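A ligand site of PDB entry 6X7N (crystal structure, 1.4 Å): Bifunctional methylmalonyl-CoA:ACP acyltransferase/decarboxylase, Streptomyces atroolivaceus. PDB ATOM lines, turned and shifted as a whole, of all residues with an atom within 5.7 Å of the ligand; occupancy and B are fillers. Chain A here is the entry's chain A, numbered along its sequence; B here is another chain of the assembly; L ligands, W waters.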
ATOM      1  N   TRP A  39      11.075 -14.117 -22.887  1.00  0.00           N
ATOM      2  CA  TRP A  39      10.500 -15.122 -21.988  1.00  0.00           C
ATOM      3  C   TRP A  39       9.641 -14.409 -20.918  1.00  0.00           C
ATOM      4  O   TRP A  39       8.597 -14.976 -20.607  1.00  0.00           O
ATOM      5  CB  TRP A  39      11.591 -15.988 -21.352  1.00  0.00           C
ATOM      6  CG  TRP A  39      12.111 -17.081 -22.255  1.00  0.00           C
ATOM      7  CD1 TRP A  39      12.017 -17.177 -23.615  1.00  0.00           C
ATOM      8  CD2 TRP A  39      12.690 -18.320 -21.799  1.00  0.00           C
ATOM      9  NE1 TRP A  39      12.552 -18.369 -24.016  1.00  0.00           N
ATOM     10  CE2 TRP A  39      12.934 -19.112 -22.934  1.00  0.00           C
ATOM     11  CE3 TRP A  39      13.004 -18.880 -20.546  1.00  0.00           C
ATOM     12  CZ2 TRP A  39      13.449 -20.413 -22.887  1.00  0.00           C
ATOM     13  CZ3 TRP A  39      13.485 -20.171 -20.486  1.00  0.00           C
ATOM     14  CH2 TRP A  39      13.779 -20.893 -21.640  1.00  0.00           C
ATOM     15  N   LEU A  63      11.190 -22.838 -24.425  1.00  0.00           N
ATOM     16  CA  LEU A  63      10.632 -21.938 -25.443  1.00  0.00           C
ATOM     17  C   LEU A  63      11.821 -21.496 -26.319  1.00  0.00           C
ATOM     18  O   LEU A  63      12.392 -20.353 -26.179  1.00  0.00           O
ATOM     19  CB  LEU A  63       9.855 -20.769 -24.840  1.00  0.00           C
ATOM     20  CG  LEU A  63       9.202 -19.881 -25.882  1.00  0.00           C
ATOM     21  CD1 LEU A  63       8.383 -20.665 -26.864  1.00  0.00           C
ATOM     22  CD2 LEU A  63       8.381 -18.802 -25.191  1.00  0.00           C
ATOM     23  N   ALA A  64      12.227 -22.352 -27.242  1.00  0.00           N
ATOM     24  CA  ALA A  64      13.532 -22.183 -27.935  1.00  0.00           C
ATOM     25  C   ALA A  64      13.467 -21.072 -28.954  1.00  0.00           C
ATOM     26  O   ALA A  64      12.506 -20.964 -29.709  1.00  0.00           O
ATOM     27  CB  ALA A  64      13.895 -23.433 -28.672  1.00  0.00           C
ATOM     28  N   PHE A  65      14.520 -20.269 -29.015  1.00  0.00           N
ATOM     29  CA  PHE A  65      14.676 -19.267 -30.080  1.00  0.00           C
ATOM     30  C   PHE A  65      14.816 -19.974 -31.420  1.00  0.00           C
ATOM     31  O   PHE A  65      15.585 -20.938 -31.459  1.00  0.00           O
ATOM     32  CB  PHE A  65      15.839 -18.336 -29.731  1.00  0.00           C
ATOM     33  CG  PHE A  65      15.500 -17.460 -28.546  1.00  0.00           C
ATOM     34  CD1 PHE A  65      15.744 -17.902 -27.243  1.00  0.00           C
ATOM     35  CD2 PHE A  65      14.898 -16.240 -28.734  1.00  0.00           C
ATOM     36  CE1 PHE A  65      15.282 -17.156 -26.160  1.00  0.00           C
ATOM     37  CE2 PHE A  65      14.489 -15.490 -27.644  1.00  0.00           C
ATOM     38  CZ  PHE A  65      14.662 -15.961 -26.376  1.00  0.00           C
ATOM     39  N   TYR A  66      14.104 -19.500 -32.418  1.00  0.00           N
ATOM     40  CA  TYR A  66      14.104 -20.142 -33.744  1.00  0.00           C
ATOM     41  C   TYR A  66      14.378 -19.104 -34.824  1.00  0.00           C
ATOM     42  O   TYR A  66      15.257 -19.370 -35.661  1.00  0.00           O
ATOM     43  CB  TYR A  66      12.812 -20.922 -33.979  1.00  0.00           C
ATOM     44  CG  TYR A  66      12.928 -21.694 -35.282  1.00  0.00           C
ATOM     45  CD1 TYR A  66      13.591 -22.894 -35.322  1.00  0.00           C
ATOM     46  CD2 TYR A  66      12.471 -21.170 -36.482  1.00  0.00           C
ATOM     47  CE1 TYR A  66      13.806 -23.614 -36.493  1.00  0.00           C
ATOM     48  CE2 TYR A  66      12.688 -21.873 -37.668  1.00  0.00           C
ATOM     49  CZ  TYR A  66      13.345 -23.071 -37.671  1.00  0.00           C
ATOM     50  OH  TYR A  66      13.623 -23.777 -38.836  1.00  0.00           O
ATOM     51  N   ASN A 139       9.658 -18.067 -31.441  1.00  0.00           N
ATOM     52  CA  ASN A 139      10.118 -19.139 -30.551  1.00  0.00           C
ATOM     53  C   ASN A 139       9.212 -20.372 -30.680  1.00  0.00           C
ATOM     54  O   ASN A 139       8.044 -20.200 -30.907  1.00  0.00           O
ATOM     55  CB  ASN A 139      10.199 -18.683 -29.099  1.00  0.00           C
ATOM     56  CG  ASN A 139      11.263 -17.627 -28.832  1.00  0.00           C
ATOM     57  OD1 ASN A 139      11.225 -16.517 -29.412  1.00  0.00           O
ATOM     58  ND2 ASN A 139      12.187 -17.922 -27.914  1.00  0.00           N
ATOM     59  N   ARG A 140       9.806 -21.542 -30.517  1.00  0.00           N
ATOM     60  CA  ARG A 140       9.116 -22.852 -30.662  1.00  0.00           C
ATOM     61  C   ARG A 140       9.379 -23.679 -29.424  1.00  0.00           C
ATOM     62  O   ARG A 140      10.493 -23.861 -28.998  1.00  0.00           O
ATOM     63  CB  ARG A 140       9.621 -23.591 -31.915  1.00  0.00           C
ATOM     64  CG  ARG A 140       9.380 -22.817 -33.199  1.00  0.00           C
ATOM     65  CD  ARG A 140      10.058 -23.402 -34.398  1.00  0.00           C
ATOM     66  NE  ARG A 140       9.394 -24.600 -34.893  1.00  0.00           N
ATOM     67  CZ  ARG A 140       9.598 -25.126 -36.092  1.00  0.00           C
ATOM     68  NH1 ARG A 140      10.413 -24.544 -36.950  1.00  0.00           N
ATOM     69  NH2 ARG A 140       8.928 -26.221 -36.418  1.00  0.00           N
ATOM     70  N   VAL A 142      10.045 -26.801 -27.322  1.00  0.00           N
ATOM     71  CA  VAL A 142      10.724 -28.082 -27.631  1.00  0.00           C
ATOM     72  C   VAL A 142      11.026 -28.830 -26.346  1.00  0.00           C
ATOM     73  O   VAL A 142      11.165 -28.222 -25.238  1.00  0.00           O
ATOM     74  CB  VAL A 142      12.022 -27.900 -28.451  1.00  0.00           C
ATOM     75  CG1 VAL A 142      11.768 -27.200 -29.765  1.00  0.00           C
ATOM     76  CG2 VAL A 142      13.088 -27.201 -27.618  1.00  0.00           C
ATOM     77  N   LEU A 153      15.468 -32.504 -31.347  1.00  0.00           N
ATOM     78  CA  LEU A 153      14.509 -31.974 -30.334  1.00  0.00           C
ATOM     79  C   LEU A 153      13.089 -32.103 -30.888  1.00  0.00           C
ATOM     80  O   LEU A 153      12.898 -32.199 -32.093  1.00  0.00           O
ATOM     81  CB  LEU A 153      14.898 -30.518 -30.045  1.00  0.00           C
ATOM     82  CG  LEU A 153      16.319 -30.253 -29.523  1.00  0.00           C
ATOM     83  CD1 LEU A 153      16.482 -28.746 -29.267  1.00  0.00           C
ATOM     84  CD2 LEU A 153      16.617 -30.999 -28.266  1.00  0.00           C
ATOM     85  N   VAL A 154      12.122 -32.160 -29.978  1.00  0.00           N
ATOM     86  CA  VAL A 154      10.718 -32.519 -30.313  1.00  0.00           C
ATOM     87  C   VAL A 154       9.763 -31.336 -30.043  1.00  0.00           C
ATOM     88  O   VAL A 154       9.886 -30.724 -28.969  1.00  0.00           O
ATOM     89  CB  VAL A 154      10.314 -33.751 -29.487  1.00  0.00           C
ATOM     90  CG1 VAL A 154       8.954 -34.276 -29.876  1.00  0.00           C
ATOM     91  CG2 VAL A 154      11.345 -34.841 -29.586  1.00  0.00           C
ATOM     92  N   LYS A 155       8.869 -31.013 -30.979  1.00  0.00           N
ATOM     93  CA  LYS A 155       7.860 -29.941 -30.813  1.00  0.00           C
ATOM     94  C   LYS A 155       7.049 -30.233 -29.553  1.00  0.00           C
ATOM     95  O   LYS A 155       6.848 -31.432 -29.131  1.00  0.00           O
ATOM     96  CB  LYS A 155       6.996 -29.732 -32.056  1.00  0.00           C
ATOM     97  CG  LYS A 155       5.867 -30.713 -32.233  1.00  0.00           C
ATOM     98  CD  LYS A 155       5.112 -30.436 -33.488  1.00  0.00           C
ATOM     99  CE  LYS A 155       3.929 -31.368 -33.585  1.00  0.00           C
ATOM    100  NZ  LYS A 155       2.941 -30.890 -34.582  1.00  0.00           N
ATOM    101  N   ARG A 183      16.714 -21.149 -44.891  1.00  0.00           N
ATOM    102  CA  ARG A 183      17.283 -22.510 -44.745  1.00  0.00           C
ATOM    103  C   ARG A 183      17.628 -23.060 -46.142  1.00  0.00           C
ATOM    104  O   ARG A 183      18.517 -23.918 -46.215  1.00  0.00           O
ATOM    105  CB  ARG A 183      16.299 -23.485 -44.092  1.00  0.00           C
ATOM    106  CG  ARG A 183      15.771 -23.020 -42.738  1.00  0.00           C
ATOM    107  CD  ARG A 183      14.890 -24.080 -42.079  1.00  0.00           C
ATOM    108  NE  ARG A 183      13.721 -24.492 -42.853  1.00  0.00           N
ATOM    109  CZ  ARG A 183      12.526 -24.856 -42.366  1.00  0.00           C
ATOM    110  NH1 ARG A 183      12.276 -24.847 -41.063  1.00  0.00           N
ATOM    111  NH2 ARG A 183      11.583 -25.252 -43.198  1.00  0.00           N
ATOM    112  N   ASN A 216      24.278 -23.235 -21.802  1.00  0.00           N
ATOM    113  CA  ASN A 216      23.237 -22.601 -20.982  1.00  0.00           C
ATOM    114  C   ASN A 216      22.905 -23.411 -19.724  1.00  0.00           C
ATOM    115  O   ASN A 216      23.530 -24.530 -19.549  1.00  0.00           O
ATOM    116  CB  ASN A 216      22.036 -22.220 -21.848  1.00  0.00           C
ATOM    117  CG  ASN A 216      21.085 -23.357 -22.167  1.00  0.00           C
ATOM    118  OD1 ASN A 216      21.269 -24.456 -21.627  1.00  0.00           O
ATOM    119  ND2 ASN A 216      20.168 -23.177 -23.076  1.00  0.00           N
ATOM    120  N   LEU A 220      22.042 -26.957 -23.115  1.00  0.00           N
ATOM    121  CA  LEU A 220      21.991 -26.712 -24.563  1.00  0.00           C
ATOM    122  C   LEU A 220      23.049 -25.660 -24.938  1.00  0.00           C
ATOM    123  O   LEU A 220      23.518 -24.885 -24.047  1.00  0.00           O
ATOM    124  CB  LEU A 220      20.617 -26.162 -24.958  1.00  0.00           C
ATOM    125  CG  LEU A 220      19.449 -27.121 -24.772  1.00  0.00           C
ATOM    126  CD1 LEU A 220      18.114 -26.361 -24.930  1.00  0.00           C
ATOM    127  CD2 LEU A 220      19.519 -28.281 -25.768  1.00  0.00           C
ATOM    128  N   LEU A 221      23.413 -25.537 -26.209  1.00  0.00           N
ATOM    129  CA  LEU A 221      24.097 -24.327 -26.687  1.00  0.00           C
ATOM    130  C   LEU A 221      23.203 -23.117 -26.431  1.00  0.00           C
ATOM    131  O   LEU A 221      22.014 -23.155 -26.791  1.00  0.00           O
ATOM    132  CB  LEU A 221      24.329 -24.444 -28.176  1.00  0.00           C
ATOM    133  CG  LEU A 221      25.357 -25.455 -28.650  1.00  0.00           C
ATOM    134  CD1 LEU A 221      25.675 -25.159 -30.102  1.00  0.00           C
ATOM    135  CD2 LEU A 221      26.603 -25.426 -27.799  1.00  0.00           C
ATOM    136  N   TYR A 222      23.796 -22.086 -25.833  1.00  0.00           N
ATOM    137  CA  TYR A 222      23.040 -20.869 -25.452  1.00  0.00           C
ATOM    138  C   TYR A 222      22.670 -20.057 -26.669  1.00  0.00           C
ATOM    139  O   TYR A 222      23.551 -19.812 -27.547  1.00  0.00           O
ATOM    140  CB  TYR A 222      23.900 -20.059 -24.497  1.00  0.00           C
ATOM    141  CG  TYR A 222      23.340 -18.760 -23.975  1.00  0.00           C
ATOM    142  CD1 TYR A 222      22.051 -18.690 -23.476  1.00  0.00           C
ATOM    143  CD2 TYR A 222      24.150 -17.665 -23.831  1.00  0.00           C
ATOM    144  CE1 TYR A 222      21.555 -17.513 -22.917  1.00  0.00           C
ATOM    145  CE2 TYR A 222      23.683 -16.483 -23.318  1.00  0.00           C
ATOM    146  CZ  TYR A 222      22.391 -16.412 -22.848  1.00  0.00           C
ATOM    147  OH  TYR A 222      21.946 -15.213 -22.323  1.00  0.00           O
ATOM    148  N   PHE A 223      21.444 -19.586 -26.737  1.00  0.00           N
ATOM    149  CA  PHE A 223      20.975 -18.922 -27.974  1.00  0.00           C
ATOM    150  C   PHE A 223      21.869 -17.729 -28.287  1.00  0.00           C
ATOM    151  O   PHE A 223      22.150 -17.424 -29.477  1.00  0.00           O
ATOM    152  CB  PHE A 223      19.496 -18.519 -27.889  1.00  0.00           C
ATOM    153  CG  PHE A 223      19.241 -17.295 -27.053  1.00  0.00           C
ATOM    154  CD1 PHE A 223      19.122 -17.397 -25.678  1.00  0.00           C
ATOM    155  CD2 PHE A 223      19.086 -16.026 -27.598  1.00  0.00           C
ATOM    156  CE1 PHE A 223      18.913 -16.286 -24.887  1.00  0.00           C
ATOM    157  CE2 PHE A 223      18.925 -14.914 -26.806  1.00  0.00           C
ATOM    158  CZ  PHE A 223      18.828 -15.033 -25.456  1.00  0.00           C
ATOM    159  N   ALA A 224      22.324 -16.979 -27.302  1.00  0.00           N
ATOM    160  CA  ALA A 224      23.114 -15.754 -27.630  1.00  0.00           C
ATOM    161  C   ALA A 224      24.484 -16.160 -28.164  1.00  0.00           C
ATOM    162  O   ALA A 224      25.090 -15.341 -28.873  1.00  0.00           O
ATOM    163  CB  ALA A 224      23.213 -14.850 -26.422  1.00  0.00           C
ATOM    164  N   TYR A 226      25.092 -18.238 -30.430  1.00  0.00           N
ATOM    165  CA  TYR A 226      25.041 -18.280 -31.916  1.00  0.00           C
ATOM    166  C   TYR A 226      25.422 -16.929 -32.507  1.00  0.00           C
ATOM    167  O   TYR A 226      26.083 -16.897 -33.584  1.00  0.00           O
ATOM    168  CB  TYR A 226      23.673 -18.701 -32.429  1.00  0.00           C
ATOM    169  CG  TYR A 226      23.327 -20.156 -32.188  1.00  0.00           C
ATOM    170  CD1 TYR A 226      23.154 -20.684 -30.934  1.00  0.00           C
ATOM    171  CD2 TYR A 226      23.018 -20.966 -33.272  1.00  0.00           C
ATOM    172  CE1 TYR A 226      22.802 -22.018 -30.738  1.00  0.00           C
ATOM    173  CE2 TYR A 226      22.652 -22.297 -33.097  1.00  0.00           C
ATOM    174  CZ  TYR A 226      22.498 -22.823 -31.830  1.00  0.00           C
ATOM    175  OH  TYR A 226      22.109 -24.125 -31.622  1.00  0.00           O
ATOM    176  N   TYR A 260      17.836 -20.541 -36.021  1.00  0.00           N
ATOM    177  CA  TYR A 260      18.344 -21.654 -35.196  1.00  0.00           C
ATOM    178  C   TYR A 260      17.750 -22.976 -35.703  1.00  0.00           C
ATOM    179  O   TYR A 260      16.701 -23.412 -35.231  1.00  0.00           O
ATOM    180  CB  TYR A 260      18.012 -21.423 -33.718  1.00  0.00           C
ATOM    181  CG  TYR A 260      18.537 -20.197 -33.048  1.00  0.00           C
ATOM    182  CD1 TYR A 260      17.892 -18.972 -33.166  1.00  0.00           C
ATOM    183  CD2 TYR A 260      19.655 -20.255 -32.261  1.00  0.00           C
ATOM    184  CE1 TYR A 260      18.382 -17.850 -32.531  1.00  0.00           C
ATOM    185  CE2 TYR A 260      20.147 -19.133 -31.611  1.00  0.00           C
ATOM    186  CZ  TYR A 260      19.498 -17.907 -31.758  1.00  0.00           C
ATOM    187  OH  TYR A 260      19.960 -16.779 -31.147  1.00  0.00           O
ATOM    188  N   LEU A 261      18.400 -23.602 -36.693  1.00  0.00           N
ATOM    189  CA  LEU A 261      17.896 -24.839 -37.345  1.00  0.00           C
ATOM    190  C   LEU A 261      18.105 -26.015 -36.390  1.00  0.00           C
ATOM    191  O   LEU A 261      17.320 -27.010 -36.441  1.00  0.00           O
ATOM    192  CB  LEU A 261      18.638 -25.143 -38.643  1.00  0.00           C
ATOM    193  CG  LEU A 261      18.423 -24.179 -39.804  1.00  0.00           C
ATOM    194  CD1 LEU A 261      17.025 -23.623 -39.746  1.00  0.00           C
ATOM    195  CD2 LEU A 261      19.461 -23.093 -39.812  1.00  0.00           C
ATOM    196  N   GLY A 262      19.123 -25.953 -35.558  1.00  0.00           N
ATOM    197  CA  GLY A 262      19.411 -27.030 -34.639  1.00  0.00           C
ATOM    198  C   GLY A 262      20.239 -26.569 -33.476  1.00  0.00           C
ATOM    199  O   GLY A 262      20.862 -25.493 -33.573  1.00  0.00           O
ATOM    200  N   ASN A 263      20.257 -27.389 -32.456  1.00  0.00           N
ATOM    201  CA  ASN A 263      21.216 -27.299 -31.337  1.00  0.00           C
ATOM    202  C   ASN A 263      22.337 -28.322 -31.552  1.00  0.00           C
ATOM    203  O   ASN A 263      22.423 -28.855 -32.665  1.00  0.00           O
ATOM    204  CB  ASN A 263      20.540 -27.411 -29.975  1.00  0.00           C
ATOM    205  CG  ASN A 263      21.223 -26.599 -28.897  1.00  0.00           C
ATOM    206  OD1 ASN A 263      22.166 -27.083 -28.300  1.00  0.00           O
ATOM    207  ND2 ASN A 263      20.721 -25.380 -28.670  1.00  0.00           N
ATOM    208  N   PRO B  21      17.472 -17.539 -18.496  1.00  0.00           N
ATOM    209  CA  PRO B  21      18.600 -17.968 -19.292  1.00  0.00           C
ATOM    210  C   PRO B  21      19.837 -17.068 -19.211  1.00  0.00           C
ATOM    211  O   PRO B  21      20.976 -17.547 -19.318  1.00  0.00           O
ATOM    212  CB  PRO B  21      18.058 -18.000 -20.728  1.00  0.00           C
ATOM    213  CG  PRO B  21      16.605 -18.335 -20.506  1.00  0.00           C
ATOM    214  CD  PRO B  21      16.233 -17.505 -19.289  1.00  0.00           C
ATOM    215  N   PHE B  83      16.910 -22.997 -15.089  1.00  0.00           N
ATOM    216  CA  PHE B  83      15.805 -22.139 -15.566  1.00  0.00           C
ATOM    217  C   PHE B  83      14.586 -22.384 -14.673  1.00  0.00           C
ATOM    218  O   PHE B  83      14.225 -23.514 -14.484  1.00  0.00           O
ATOM    219  CB  PHE B  83      15.426 -22.468 -17.004  1.00  0.00           C
ATOM    220  CG  PHE B  83      16.463 -22.220 -18.080  1.00  0.00           C
ATOM    221  CD1 PHE B  83      17.704 -21.648 -17.810  1.00  0.00           C
ATOM    222  CD2 PHE B  83      16.157 -22.489 -19.412  1.00  0.00           C
ATOM    223  CE1 PHE B  83      18.638 -21.446 -18.817  1.00  0.00           C
ATOM    224  CE2 PHE B  83      17.092 -22.246 -20.418  1.00  0.00           C
ATOM    225  CZ  PHE B  83      18.343 -21.777 -20.102  1.00  0.00           C
HETATM  226  O1  LIG L   1       9.041 -30.795 -38.550  1.00  0.00           O
HETATM  227  P1  LIG L   1       9.940 -30.727 -37.174  1.00  0.00           P
HETATM  228  O2  LIG L   1      10.636 -32.030 -36.865  1.00  0.00           O
HETATM  229  O3  LIG L   1       9.215 -30.094 -36.039  1.00  0.00           O
HETATM  230  O4  LIG L   1      11.107 -29.720 -37.608  1.00  0.00           O
HETATM  231  P2  LIG L   1      12.655 -29.819 -37.285  1.00  0.00           P
HETATM  232  O5  LIG L   1      13.228 -28.748 -38.196  1.00  0.00           O
HETATM  233  O6  LIG L   1      13.442 -31.151 -37.246  1.00  0.00           O
HETATM  234  O7  LIG L   1      12.772 -29.336 -35.715  1.00  0.00           O
HETATM  235  C1  LIG L   1      12.235 -28.102 -35.341  1.00  0.00           C
HETATM  236  C2  LIG L   1      13.159 -27.719 -34.173  1.00  0.00           C
HETATM  237  C3  LIG L   1      13.063 -28.813 -33.118  1.00  0.00           C
HETATM  238  C4  LIG L   1      12.661 -26.393 -33.558  1.00  0.00           C
HETATM  239  C5  LIG L   1      14.617 -27.593 -34.659  1.00  0.00           C
HETATM  240  O8  LIG L   1      14.706 -26.658 -35.753  1.00  0.00           O
HETATM  241  C6  LIG L   1      15.594 -27.170 -33.538  1.00  0.00           C
HETATM  242  O9  LIG L   1      16.014 -27.958 -32.741  1.00  0.00           O
HETATM  243  N1  LIG L   1      16.064 -25.918 -33.559  1.00  0.00           N
HETATM  244  C7  LIG L   1      17.095 -25.431 -32.658  1.00  0.00           C
HETATM  245  C8  LIG L   1      16.505 -24.427 -31.642  1.00  0.00           C
HETATM  246  C9  LIG L   1      17.580 -23.975 -30.698  1.00  0.00           C
HETATM  247  O10 LIG L   1      18.413 -24.753 -30.275  1.00  0.00           O
HETATM  248  N2  LIG L   1      17.507 -22.737 -30.263  1.00  0.00           N
HETATM  249  C10 LIG L   1      18.293 -22.087 -29.188  1.00  0.00           C
HETATM  250  C11 LIG L   1      18.175 -22.879 -27.886  1.00  0.00           C
HETATM  251  N3  LIG L   1      18.454 -22.044 -26.789  1.00  0.00           N
HETATM  252  C12 LIG L   1      17.440 -21.250 -26.275  1.00  0.00           C
HETATM  253  O11 LIG L   1      16.360 -21.113 -26.843  1.00  0.00           O
HETATM  254  C13 LIG L   1      17.601 -20.689 -24.893  1.00  0.00           C
HETATM  255  C14 LIG L   1      16.472 -19.921 -24.250  1.00  0.00           C
HETATM  256  N4  LIG L   1      18.801 -20.678 -24.279  1.00  0.00           N
HETATM  257  O12 LIG L   1      18.984 -20.015 -23.111  1.00  0.00           O
HETATM  258  O13 LIG L   1      19.909 -21.019 -24.899  1.00  0.00           O
HETATM  259  O   HOH W   1      16.366 -31.330 -35.643  1.00  0.00           O
HETATM  260  O   HOH W   2      14.700 -26.317 -38.795  1.00  0.00           O
HETATM  261  O   HOH W   3      14.706 -30.085 -40.259  1.00  0.00           O
HETATM  262  O   HOH W   4      14.120 -32.532 -34.561  1.00  0.00           O
HETATM  263  O   HOH W   5      16.605 -30.479 -33.142  1.00  0.00           O
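Water W5 lies within hydrogen-bond range of an oxygen (O9) of the ligand and the backbone NH of Leu 153.
Water W2 bridges the side-chain hydroxyl (OH) of Tyr 66 and an oxygen (O5) of the ligand.
Water W4 lies within hydrogen-bond range of O of Leu 153 (2.8 Å) and O6 of the ligand (3.1 Å).
Merely in contact with the ligand: Tyr 222 (3.2 Å), Ala 64 (3.2 Å), Pro 21 of chain B (3.3 Å), Tyr 66 (3.3 Å), Trp 39 (3.4 Å), Gly 262 (3.4 Å), Leu 153 (3.5 Å), Phe 83 of chain B (3.5 Å), Leu 221 (3.5 Å), Val 142 (3.9 Å) and Tyr 226 (3.98 Å).
Hydrophobic or aromatic side chains that line the ligand: Trp 39, Ala 64, Phe 65, Tyr 66, Val 142, Leu 153, Tyr 222, Phe 223, Tyr 260, Pro 21 of chain B and Phe 83 of chain B.
O8 of the ligand sits at hydrogen-bond distance from O of Leu 261 (2.7 Å).
The backbone NH (N) of Phe 223 sits at hydrogen-bond distance from an oxygen (O13) of the ligand.
ND2 of Asn 216 lies within hydrogen-bond range of O13 of the ligand (2.8 Å).
O10 of the ligand is in hydrogen-bond range of ND2 of Asn 263 (2.9 Å).
N of Phe 65 lies within hydrogen-bond range of O11 of the ligand (3.0 Å).
The backbone carbonyl oxygen of Phe 65 is in hydrogen-bond range of a nitrogen (N2) of the ligand.
The backbone carbonyl oxygen (O) of Tyr 260 is in hydrogen-bond range of a nitrogen (N1) of the ligand (3.1 Å).
The guanidinium group of Arg 140 is in salt-bridge range of an oxygen (O3) of the ligand (3.9 Å).
The backbone carbonyl oxygen of Phe 223 sits at hydrogen-bond distance from the side-chain hydroxyl of Tyr 260 (2.8 Å).
OD1 of Asn 216 is in hydrogen-bond range of N of Leu 220, at 3.0 Å.
The side-chain amide oxygen (OD1) of Asn 263 sits at hydrogen-bond distance from the backbone NH (N) of Leu 221 (2.9 Å).
The backbone NH (N) of Tyr 260 sits at hydrogen-bond distance from the backbone carbonyl oxygen (O) of Tyr 66, 2.9 Å away.
O of Ala 64 is in hydrogen-bond range of N of Arg 140.
The side-chain hydroxyl (OH) of Tyr 66 sits at hydrogen-bond distance from the guanidinium group (NH1) of Arg 183 (2.8 Å).
The indole nitrogen of Trp 39 is in hydrogen-bond range of the backbone carbonyl oxygen of Leu 63 (2.9 Å).
OH of Tyr 226 is in hydrogen-bond range of O of Gly 262 (2.7 Å).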
